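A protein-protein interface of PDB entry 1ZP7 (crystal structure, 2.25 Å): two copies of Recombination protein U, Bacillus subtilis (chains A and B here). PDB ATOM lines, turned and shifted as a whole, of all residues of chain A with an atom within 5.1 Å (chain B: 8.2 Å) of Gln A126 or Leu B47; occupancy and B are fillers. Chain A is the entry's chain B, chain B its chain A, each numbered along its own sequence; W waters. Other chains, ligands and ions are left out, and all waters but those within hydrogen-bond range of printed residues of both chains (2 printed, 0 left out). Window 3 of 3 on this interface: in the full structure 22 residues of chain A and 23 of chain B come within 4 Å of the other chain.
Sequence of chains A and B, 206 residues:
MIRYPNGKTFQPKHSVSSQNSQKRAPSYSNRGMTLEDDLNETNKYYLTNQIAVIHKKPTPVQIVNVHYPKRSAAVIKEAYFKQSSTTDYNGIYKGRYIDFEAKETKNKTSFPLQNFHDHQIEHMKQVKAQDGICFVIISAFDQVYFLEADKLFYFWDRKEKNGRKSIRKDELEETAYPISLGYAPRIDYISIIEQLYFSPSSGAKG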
ATOM      1  N   GLU A 122      19.671  13.951  -9.685  1.00  0.00           N
ATOM      2  CA  GLU A 122      20.597  15.032  -9.331  1.00  0.00           C
ATOM      3  C   GLU A 122      19.849  16.362  -9.134  1.00  0.00           C
ATOM      4  O   GLU A 122      20.118  17.093  -8.177  1.00  0.00           O
ATOM      5  CB  GLU A 122      21.757  15.129 -10.352  1.00  0.00           C
ATOM      6  CG  GLU A 122      22.820  16.218 -10.068  1.00  0.00           C
ATOM      7  CD  GLU A 122      23.610  16.030  -8.753  1.00  0.00           C
ATOM      8  OE1 GLU A 122      23.806  14.867  -8.293  1.00  0.00           O
ATOM      9  OE2 GLU A 122      24.049  17.068  -8.193  1.00  0.00           O
ATOM     10  N   HIS A 123      18.868  16.635  -9.998  1.00  0.00           N
ATOM     11  CA  HIS A 123      17.969  17.797  -9.813  1.00  0.00           C
ATOM     12  C   HIS A 123      17.277  17.785  -8.432  1.00  0.00           C
ATOM     13  O   HIS A 123      17.261  18.794  -7.723  1.00  0.00           O
ATOM     14  CB  HIS A 123      16.942  17.894 -10.948  1.00  0.00           C
ATOM     15  CG  HIS A 123      15.925  18.976 -10.744  1.00  0.00           C
ATOM     16  ND1 HIS A 123      14.654  18.726 -10.260  1.00  0.00           N
ATOM     17  CD2 HIS A 123      16.000  20.318 -10.927  1.00  0.00           C
ATOM     18  CE1 HIS A 123      13.996  19.868 -10.158  1.00  0.00           C
ATOM     19  NE2 HIS A 123      14.790  20.846 -10.559  1.00  0.00           N
ATOM     20  N   MET A 124      16.733  16.630  -8.053  1.00  0.00           N
ATOM     21  CA  MET A 124      16.071  16.447  -6.745  1.00  0.00           C
ATOM     22  C   MET A 124      16.984  16.731  -5.545  1.00  0.00           C
ATOM     23  O   MET A 124      16.581  17.395  -4.590  1.00  0.00           O
ATOM     24  CB  MET A 124      15.435  15.040  -6.644  1.00  0.00           C
ATOM     25  CG  MET A 124      14.355  14.756  -7.695  1.00  0.00           C
ATOM     26  SD  MET A 124      13.424  13.217  -7.436  1.00  0.00           S
ATOM     27  CE  MET A 124      13.464  12.556  -9.096  1.00  0.00           C
ATOM     28  N   LYS A 125      18.222  16.245  -5.607  1.00  0.00           N
ATOM     29  CA  LYS A 125      19.232  16.530  -4.558  1.00  0.00           C
ATOM     30  C   LYS A 125      19.506  18.019  -4.442  1.00  0.00           C
ATOM     31  O   LYS A 125      19.578  18.557  -3.339  1.00  0.00           O
ATOM     32  CB  LYS A 125      20.553  15.789  -4.851  1.00  0.00           C
ATOM     33  CG  LYS A 125      20.491  14.294  -4.695  1.00  0.00           C
ATOM     34  CD  LYS A 125      21.678  13.646  -5.402  1.00  0.00           C
ATOM     35  CE  LYS A 125      21.450  12.151  -5.642  1.00  0.00           C
ATOM     36  NZ  LYS A 125      21.589  11.338  -4.396  1.00  0.00           N
ATOM     37  N   GLN A 126      19.647  18.683  -5.594  1.00  0.00           N
ATOM     38  CA  GLN A 126      19.842  20.134  -5.623  1.00  0.00           C
ATOM     39  C   GLN A 126      18.673  20.881  -4.995  1.00  0.00           C
ATOM     40  O   GLN A 126      18.884  21.798  -4.204  1.00  0.00           O
ATOM     41  CB  GLN A 126      20.060  20.619  -7.049  1.00  0.00           C
ATOM     42  CG  GLN A 126      21.349  20.157  -7.674  1.00  0.00           C
ATOM     43  CD  GLN A 126      21.308  20.294  -9.176  1.00  0.00           C
ATOM     44  OE1 GLN A 126      20.601  21.145  -9.704  1.00  0.00           O
ATOM     45  NE2 GLN A 126      22.054  19.440  -9.879  1.00  0.00           N
ATOM     46  N   VAL A 127      17.442  20.482  -5.332  1.00  0.00           N
ATOM     47  CA  VAL A 127      16.243  21.119  -4.747  1.00  0.00           C
ATOM     48  C   VAL A 127      16.216  20.928  -3.226  1.00  0.00           C
ATOM     49  O   VAL A 127      15.975  21.846  -2.476  1.00  0.00           O
ATOM     50  CB  VAL A 127      14.934  20.553  -5.381  1.00  0.00           C
ATOM     51  CG1 VAL A 127      13.688  21.047  -4.620  1.00  0.00           C
ATOM     52  CG2 VAL A 127      14.852  20.927  -6.855  1.00  0.00           C
ATOM     53  N   LYS A 128      16.435  19.703  -2.788  1.00  0.00           N
ATOM     54  CA  LYS A 128      16.502  19.374  -1.360  1.00  0.00           C
ATOM     55  C   LYS A 128      17.589  20.235  -0.668  1.00  0.00           C
ATOM     56  O   LYS A 128      17.306  20.969   0.267  1.00  0.00           O
ATOM     57  CB  LYS A 128      16.736  17.853  -1.225  1.00  0.00           C
ATOM     58  CG  LYS A 128      16.969  17.309   0.192  1.00  0.00           C
ATOM     59  CD  LYS A 128      15.779  17.457   1.126  1.00  0.00           C
ATOM     60  CE  LYS A 128      15.820  16.390   2.258  1.00  0.00           C
ATOM     61  NZ  LYS A 128      17.187  16.235   2.874  1.00  0.00           N
ATOM     62  N   ALA A 129      18.807  20.204  -1.194  1.00  0.00           N
ATOM     63  CA  ALA A 129      19.899  21.064  -0.688  1.00  0.00           C
ATOM     64  C   ALA A 129      19.578  22.575  -0.691  1.00  0.00           C
ATOM     65  O   ALA A 129      20.105  23.332   0.146  1.00  0.00           O
ATOM     66  CB  ALA A 129      21.192  20.771  -1.449  1.00  0.00           C
ATOM     67  N   GLN A 130      18.699  23.019  -1.603  1.00  0.00           N
ATOM     68  CA  GLN A 130      18.247  24.422  -1.619  1.00  0.00           C
ATOM     69  C   GLN A 130      17.115  24.668  -0.633  1.00  0.00           C
ATOM     70  O   GLN A 130      16.529  25.748  -0.608  1.00  0.00           O
ATOM     71  CB  GLN A 130      17.846  24.856  -3.038  1.00  0.00           C
ATOM     72  CG  GLN A 130      19.015  24.906  -4.007  1.00  0.00           C
ATOM     73  CD  GLN A 130      19.766  26.225  -3.955  1.00  0.00           C
ATOM     74  OE1 GLN A 130      19.275  27.207  -3.385  1.00  0.00           O
ATOM     75  NE2 GLN A 130      20.951  26.264  -4.573  1.00  0.00           N
ATOM     76  N   ASN B  40      19.636  32.238 -19.874  1.00  0.00           N
ATOM     77  CA  ASN B  40      20.034  30.839 -19.916  1.00  0.00           C
ATOM     78  C   ASN B  40      21.455  30.663 -19.332  1.00  0.00           C
ATOM     79  O   ASN B  40      21.693  29.814 -18.474  1.00  0.00           O
ATOM     80  CB  ASN B  40      19.915  30.338 -21.359  1.00  0.00           C
ATOM     81  CG  ASN B  40      20.369  28.926 -21.537  1.00  0.00           C
ATOM     82  OD1 ASN B  40      21.452  28.679 -22.062  1.00  0.00           O
ATOM     83  ND2 ASN B  40      19.544  27.977 -21.129  1.00  0.00           N
ATOM     84  N   GLU B  41      22.370  31.522 -19.764  1.00  0.00           N
ATOM     85  CA  GLU B  41      23.709  31.569 -19.252  1.00  0.00           C
ATOM     86  C   GLU B  41      23.734  31.996 -17.784  1.00  0.00           C
ATOM     87  O   GLU B  41      24.568  31.536 -17.012  1.00  0.00           O
ATOM     88  CB  GLU B  41      24.528  32.548 -20.103  1.00  0.00           C
ATOM     89  CG  GLU B  41      25.896  32.019 -20.529  1.00  0.00           C
ATOM     90  CD  GLU B  41      25.858  30.606 -21.164  1.00  0.00           C
ATOM     91  OE1 GLU B  41      26.744  29.797 -20.807  1.00  0.00           O
ATOM     92  OE2 GLU B  41      24.956  30.302 -21.989  1.00  0.00           O
ATOM     93  N   THR B  42      22.835  32.898 -17.408  1.00  0.00           N
ATOM     94  CA  THR B  42      22.729  33.354 -16.036  1.00  0.00           C
ATOM     95  C   THR B  42      22.303  32.193 -15.128  1.00  0.00           C
ATOM     96  O   THR B  42      22.919  31.936 -14.078  1.00  0.00           O
ATOM     97  CB  THR B  42      21.745  34.541 -15.948  1.00  0.00           C
ATOM     98  OG1 THR B  42      22.325  35.665 -16.605  1.00  0.00           O
ATOM     99  CG2 THR B  42      21.442  34.924 -14.499  1.00  0.00           C
ATOM    100  N   ASN B  43      21.258  31.497 -15.555  1.00  0.00           N
ATOM    101  CA  ASN B  43      20.657  30.423 -14.788  1.00  0.00           C
ATOM    102  C   ASN B  43      21.584  29.198 -14.706  1.00  0.00           C
ATOM    103  O   ASN B  43      21.669  28.542 -13.658  1.00  0.00           O
ATOM    104  CB  ASN B  43      19.243  30.082 -15.321  1.00  0.00           C
ATOM    105  CG  ASN B  43      18.189  31.203 -15.030  1.00  0.00           C
ATOM    106  OD1 ASN B  43      18.244  31.914 -14.008  1.00  0.00           O
ATOM    107  ND2 ASN B  43      17.218  31.318 -15.902  1.00  0.00           N
ATOM    108  N   LYS B  44      22.283  28.915 -15.802  1.00  0.00           N
ATOM    109  CA  LYS B  44      23.379  27.933 -15.817  1.00  0.00           C
ATOM    110  C   LYS B  44      24.453  28.275 -14.797  1.00  0.00           C
ATOM    111  O   LYS B  44      24.864  27.420 -14.026  1.00  0.00           O
ATOM    112  CB  LYS B  44      24.066  27.926 -17.177  1.00  0.00           C
ATOM    113  CG  LYS B  44      23.549  26.946 -18.168  1.00  0.00           C
ATOM    114  CD  LYS B  44      24.527  26.954 -19.333  1.00  0.00           C
ATOM    115  CE  LYS B  44      24.017  26.179 -20.534  1.00  0.00           C
ATOM    116  NZ  LYS B  44      22.839  26.834 -21.147  1.00  0.00           N
ATOM    117  N   TYR B  45      24.923  29.521 -14.815  1.00  0.00           N
ATOM    118  CA  TYR B  45      25.871  29.992 -13.828  1.00  0.00           C
ATOM    119  C   TYR B  45      25.400  29.756 -12.381  1.00  0.00           C
ATOM    120  O   TYR B  45      26.171  29.238 -11.550  1.00  0.00           O
ATOM    121  CB  TYR B  45      26.198  31.464 -14.045  1.00  0.00           C
ATOM    122  CG  TYR B  45      27.126  32.026 -12.995  1.00  0.00           C
ATOM    123  CD1 TYR B  45      28.510  31.899 -13.116  1.00  0.00           C
ATOM    124  CD2 TYR B  45      26.619  32.663 -11.874  1.00  0.00           C
ATOM    125  CE1 TYR B  45      29.366  32.401 -12.134  1.00  0.00           C
ATOM    126  CE2 TYR B  45      27.451  33.181 -10.893  1.00  0.00           C
ATOM    127  CZ  TYR B  45      28.827  33.040 -11.028  1.00  0.00           C
ATOM    128  OH  TYR B  45      29.644  33.565 -10.048  1.00  0.00           O
ATOM    129  N   TYR B  46      24.164  30.166 -12.072  1.00  0.00           N
ATOM    130  CA  TYR B  46      23.602  29.983 -10.728  1.00  0.00           C
ATOM    131  C   TYR B  46      23.540  28.499 -10.374  1.00  0.00           C
ATOM    132  O   TYR B  46      23.857  28.121  -9.253  1.00  0.00           O
ATOM    133  CB  TYR B  46      22.205  30.601 -10.584  1.00  0.00           C
ATOM    134  CG  TYR B  46      22.113  32.119 -10.610  1.00  0.00           C
ATOM    135  CD1 TYR B  46      23.038  32.919  -9.912  1.00  0.00           C
ATOM    136  CD2 TYR B  46      21.069  32.759 -11.301  1.00  0.00           C
ATOM    137  CE1 TYR B  46      22.937  34.306  -9.912  1.00  0.00           C
ATOM    138  CE2 TYR B  46      20.956  34.169 -11.293  1.00  0.00           C
ATOM    139  CZ  TYR B  46      21.903  34.927 -10.619  1.00  0.00           C
ATOM    140  OH  TYR B  46      21.809  36.305 -10.601  1.00  0.00           O
ATOM    141  N   LEU B  47      23.144  27.668 -11.333  1.00  0.00           N
ATOM    142  CA  LEU B  47      23.102  26.229 -11.127  1.00  0.00           C
ATOM    143  C   LEU B  47      24.483  25.642 -10.794  1.00  0.00           C
ATOM    144  O   LEU B  47      24.662  25.038  -9.729  1.00  0.00           O
ATOM    145  CB  LEU B  47      22.480  25.499 -12.325  1.00  0.00           C
ATOM    146  CG  LEU B  47      22.066  24.023 -12.062  1.00  0.00           C
ATOM    147  CD1 LEU B  47      20.791  23.959 -11.246  1.00  0.00           C
ATOM    148  CD2 LEU B  47      21.888  23.199 -13.341  1.00  0.00           C
ATOM    149  N   THR B  48      25.452  25.838 -11.693  1.00  0.00           N
ATOM    150  CA  THR B  48      26.786  25.246 -11.528  1.00  0.00           C
ATOM    151  C   THR B  48      27.553  25.774 -10.315  1.00  0.00           C
ATOM    152  O   THR B  48      28.514  25.158  -9.883  1.00  0.00           O
ATOM    153  CB  THR B  48      27.652  25.340 -12.804  1.00  0.00           C
ATOM    154  OG1 THR B  48      27.987  26.704 -13.061  1.00  0.00           O
ATOM    155  CG2 THR B  48      26.892  24.786 -13.991  1.00  0.00           C
ATOM    156  N   ASN B  49      27.128  26.906  -9.775  1.00  0.00           N
ATOM    157  CA  ASN B  49      27.755  27.476  -8.600  1.00  0.00           C
ATOM    158  C   ASN B  49      26.896  27.270  -7.356  1.00  0.00           C
ATOM    159  O   ASN B  49      27.199  27.827  -6.289  1.00  0.00           O
ATOM    160  CB  ASN B  49      28.033  28.973  -8.797  1.00  0.00           C
ATOM    161  CG  ASN B  49      29.240  29.232  -9.681  1.00  0.00           C
ATOM    162  OD1 ASN B  49      30.384  29.136  -9.232  1.00  0.00           O
ATOM    163  ND2 ASN B  49      28.996  29.574 -10.932  1.00  0.00           N
ATOM    164  N   GLN B  50      25.823  26.497  -7.509  1.00  0.00           N
ATOM    165  CA  GLN B  50      24.913  26.130  -6.403  1.00  0.00           C
ATOM    166  C   GLN B  50      24.278  27.310  -5.714  1.00  0.00           C
ATOM    167  O   GLN B  50      23.949  27.243  -4.533  1.00  0.00           O
ATOM    168  CB  GLN B  50      25.599  25.211  -5.373  1.00  0.00           C
ATOM    169  CG  GLN B  50      26.018  23.842  -5.954  1.00  0.00           C
ATOM    170  CD  GLN B  50      27.376  23.870  -6.636  1.00  0.00           C
ATOM    171  OE1 GLN B  50      28.283  24.581  -6.196  1.00  0.00           O
ATOM    172  NE2 GLN B  50      27.528  23.097  -7.699  1.00  0.00           N
ATOM    173  N   ILE B  51      24.063  28.386  -6.467  1.00  0.00           N
ATOM    174  CA  ILE B  51      23.403  29.577  -5.913  1.00  0.00           C
ATOM    175  C   ILE B  51      21.866  29.437  -5.907  1.00  0.00           C
ATOM    176  O   ILE B  51      21.208  29.774  -4.931  1.00  0.00           O
ATOM    177  CB  ILE B  51      23.893  30.868  -6.626  1.00  0.00           C
ATOM    178  CG1 ILE B  51      25.397  31.057  -6.375  1.00  0.00           C
ATOM    179  CG2 ILE B  51      23.165  32.077  -6.096  1.00  0.00           C
ATOM    180  CD1 ILE B  51      26.128  31.862  -7.445  1.00  0.00           C
ATOM    181  N   ALA B  52      21.302  28.938  -7.001  1.00  0.00           N
ATOM    182  CA  ALA B  52      19.863  28.747  -7.120  1.00  0.00           C
ATOM    183  C   ALA B  52      19.638  27.703  -8.188  1.00  0.00           C
ATOM    184  O   ALA B  52      20.541  27.397  -8.962  1.00  0.00           O
ATOM    185  CB  ALA B  52      19.155  30.070  -7.469  1.00  0.00           C
ATOM    186  N   VAL B  53      18.435  27.144  -8.214  1.00  0.00           N
ATOM    187  CA  VAL B  53      18.049  26.147  -9.196  1.00  0.00           C
ATOM    188  C   VAL B  53      16.792  26.649  -9.963  1.00  0.00           C
ATOM    189  O   VAL B  53      15.645  26.388  -9.573  1.00  0.00           O
ATOM    190  CB  VAL B  53      17.808  24.757  -8.534  1.00  0.00           C
ATOM    191  CG1 VAL B  53      17.522  23.740  -9.582  1.00  0.00           C
ATOM    192  CG2 VAL B  53      19.034  24.319  -7.686  1.00  0.00           C
ATOM    193  N   ILE B  54      17.039  27.353 -11.063  1.00  0.00           N
ATOM    194  CA  ILE B  54      15.999  28.058 -11.806  1.00  0.00           C
ATOM    195  C   ILE B  54      16.110  27.636 -13.262  1.00  0.00           C
ATOM    196  O   ILE B  54      17.206  27.627 -13.823  1.00  0.00           O
ATOM    197  CB  ILE B  54      16.150  29.612 -11.621  1.00  0.00           C
ATOM    198  CG1 ILE B  54      15.868  29.972 -10.147  1.00  0.00           C
ATOM    199  CG2 ILE B  54      15.265  30.392 -12.619  1.00  0.00           C
ATOM    200  CD1 ILE B  54      16.309  31.289  -9.688  1.00  0.00           C
ATOM    201  N   HIS B  55      14.986  27.268 -13.867  1.00  0.00           N
ATOM    202  CA  HIS B  55      14.961  26.807 -15.253  1.00  0.00           C
ATOM    203  C   HIS B  55      13.872  27.504 -16.058  1.00  0.00           C
ATOM    204  O   HIS B  55      12.824  27.839 -15.526  1.00  0.00           O
ATOM    205  CB  HIS B  55      14.726  25.289 -15.310  1.00  0.00           C
ATOM    206  CG  HIS B  55      15.868  24.487 -14.781  1.00  0.00           C
ATOM    207  ND1 HIS B  55      16.068  24.271 -13.433  1.00  0.00           N
ATOM    208  CD2 HIS B  55      16.895  23.877 -15.415  1.00  0.00           C
ATOM    209  CE1 HIS B  55      17.168  23.565 -13.259  1.00  0.00           C
ATOM    210  NE2 HIS B  55      17.683  23.302 -14.446  1.00  0.00           N
ATOM    211  N   ILE B  92      14.005  27.683  -7.337  1.00  0.00           N
ATOM    212  CA  ILE B  92      14.165  27.813  -5.889  1.00  0.00           C
ATOM    213  C   ILE B  92      15.424  28.574  -5.542  1.00  0.00           C
ATOM    214  O   ILE B  92      16.470  28.340  -6.135  1.00  0.00           O
ATOM    215  CB  ILE B  92      14.161  26.403  -5.195  1.00  0.00           C
ATOM    216  CG1 ILE B  92      14.113  26.525  -3.663  1.00  0.00           C
ATOM    217  CG2 ILE B  92      15.303  25.509  -5.698  1.00  0.00           C
ATOM    218  CD1 ILE B  92      14.217  25.195  -2.956  1.00  0.00           C
HETATM  219  O   HOH W   1      18.447  21.333 -11.729  1.00  0.00           O
HETATM  220  O   HOH W   2      13.925  24.199 -10.141  1.00  0.00           O
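Water W2 lies within hydrogen-bond range of O of Val B53 (2.8 Å) and NE2 of His A123 (3.5 Å).
Water W1 lies within hydrogen-bond range of OE1 of Gln A126 (3.0 Å) and NE2 of His B55 (3.4 Å).
The backbone carbonyl oxygen (O) of Gln B50 lies within hydrogen-bond range of the side-chain amide nitrogen (NE2) of Gln A130 (3.2 Å).
No position is printed for both chains.
Of the 9 pairs that touch across the chains among the printed residues, none has its exchanged pair printed and touching as well.
His A123 touches Val B53.
Leu B47 touches Gln A126 (CD1 to OE1, 3.2 Å).
Gln A126 touches Val B53.
Ile B92 touches Val A127.
Ile B51 touches Gln A130.
Ala B52 touches Gln A130 (N to NE2, 3.6 Å).
Val B53 touches Gln A130.
Gln A130 touches Ile B92 (O to CD1, 3.3 Å).
O of Tyr B46 lies within hydrogen-bond range of N of Ile B51, 2.8 Å away.
The backbone carbonyl oxygen of Thr B48 sits at hydrogen-bond distance from the side-chain amide nitrogen of Gln B50 (3.2 Å).
O of Val B53 sits at hydrogen-bond distance from N of Ile B92.
O of Glu A122 lies close to NE2 of Gln A126 (3.5 Å).
Of the 9 printed residues of chain A, 4 touch a printed residue of chain B.
Hydrophobic or aromatic side chains of chain A within 4 Å of the printed part of chain B: His A123.
Among the printed residues, 9 pairs touch across the chains.
Gln A126 touches just these residues of chain B: Leu B47 and Val B53.
Of the printed residues of chain B, Gln A130 touches Gln B50 (3.2 Å), Ile B51 (3.5 Å), Ala B52 (3.6 Å), Val B53 (3.7 Å) and Ile B92 (3.3 Å).
Printed residues of chain A within 4 Å of Ala B52: Gln A130.
Printed residues of chain B within 4 Å of Val A127: Ile B92.
Glu B41 touches none of the printed residues of chain A.
Thr B48 touches none of the printed residues of chain A.
The nearest residue of chain B that does not touch Gln A126 is Ile B92 (5.4 Å).
The nearest printed residue of chain A that does not touch Leu B47 is His A123 (6.0 Å).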
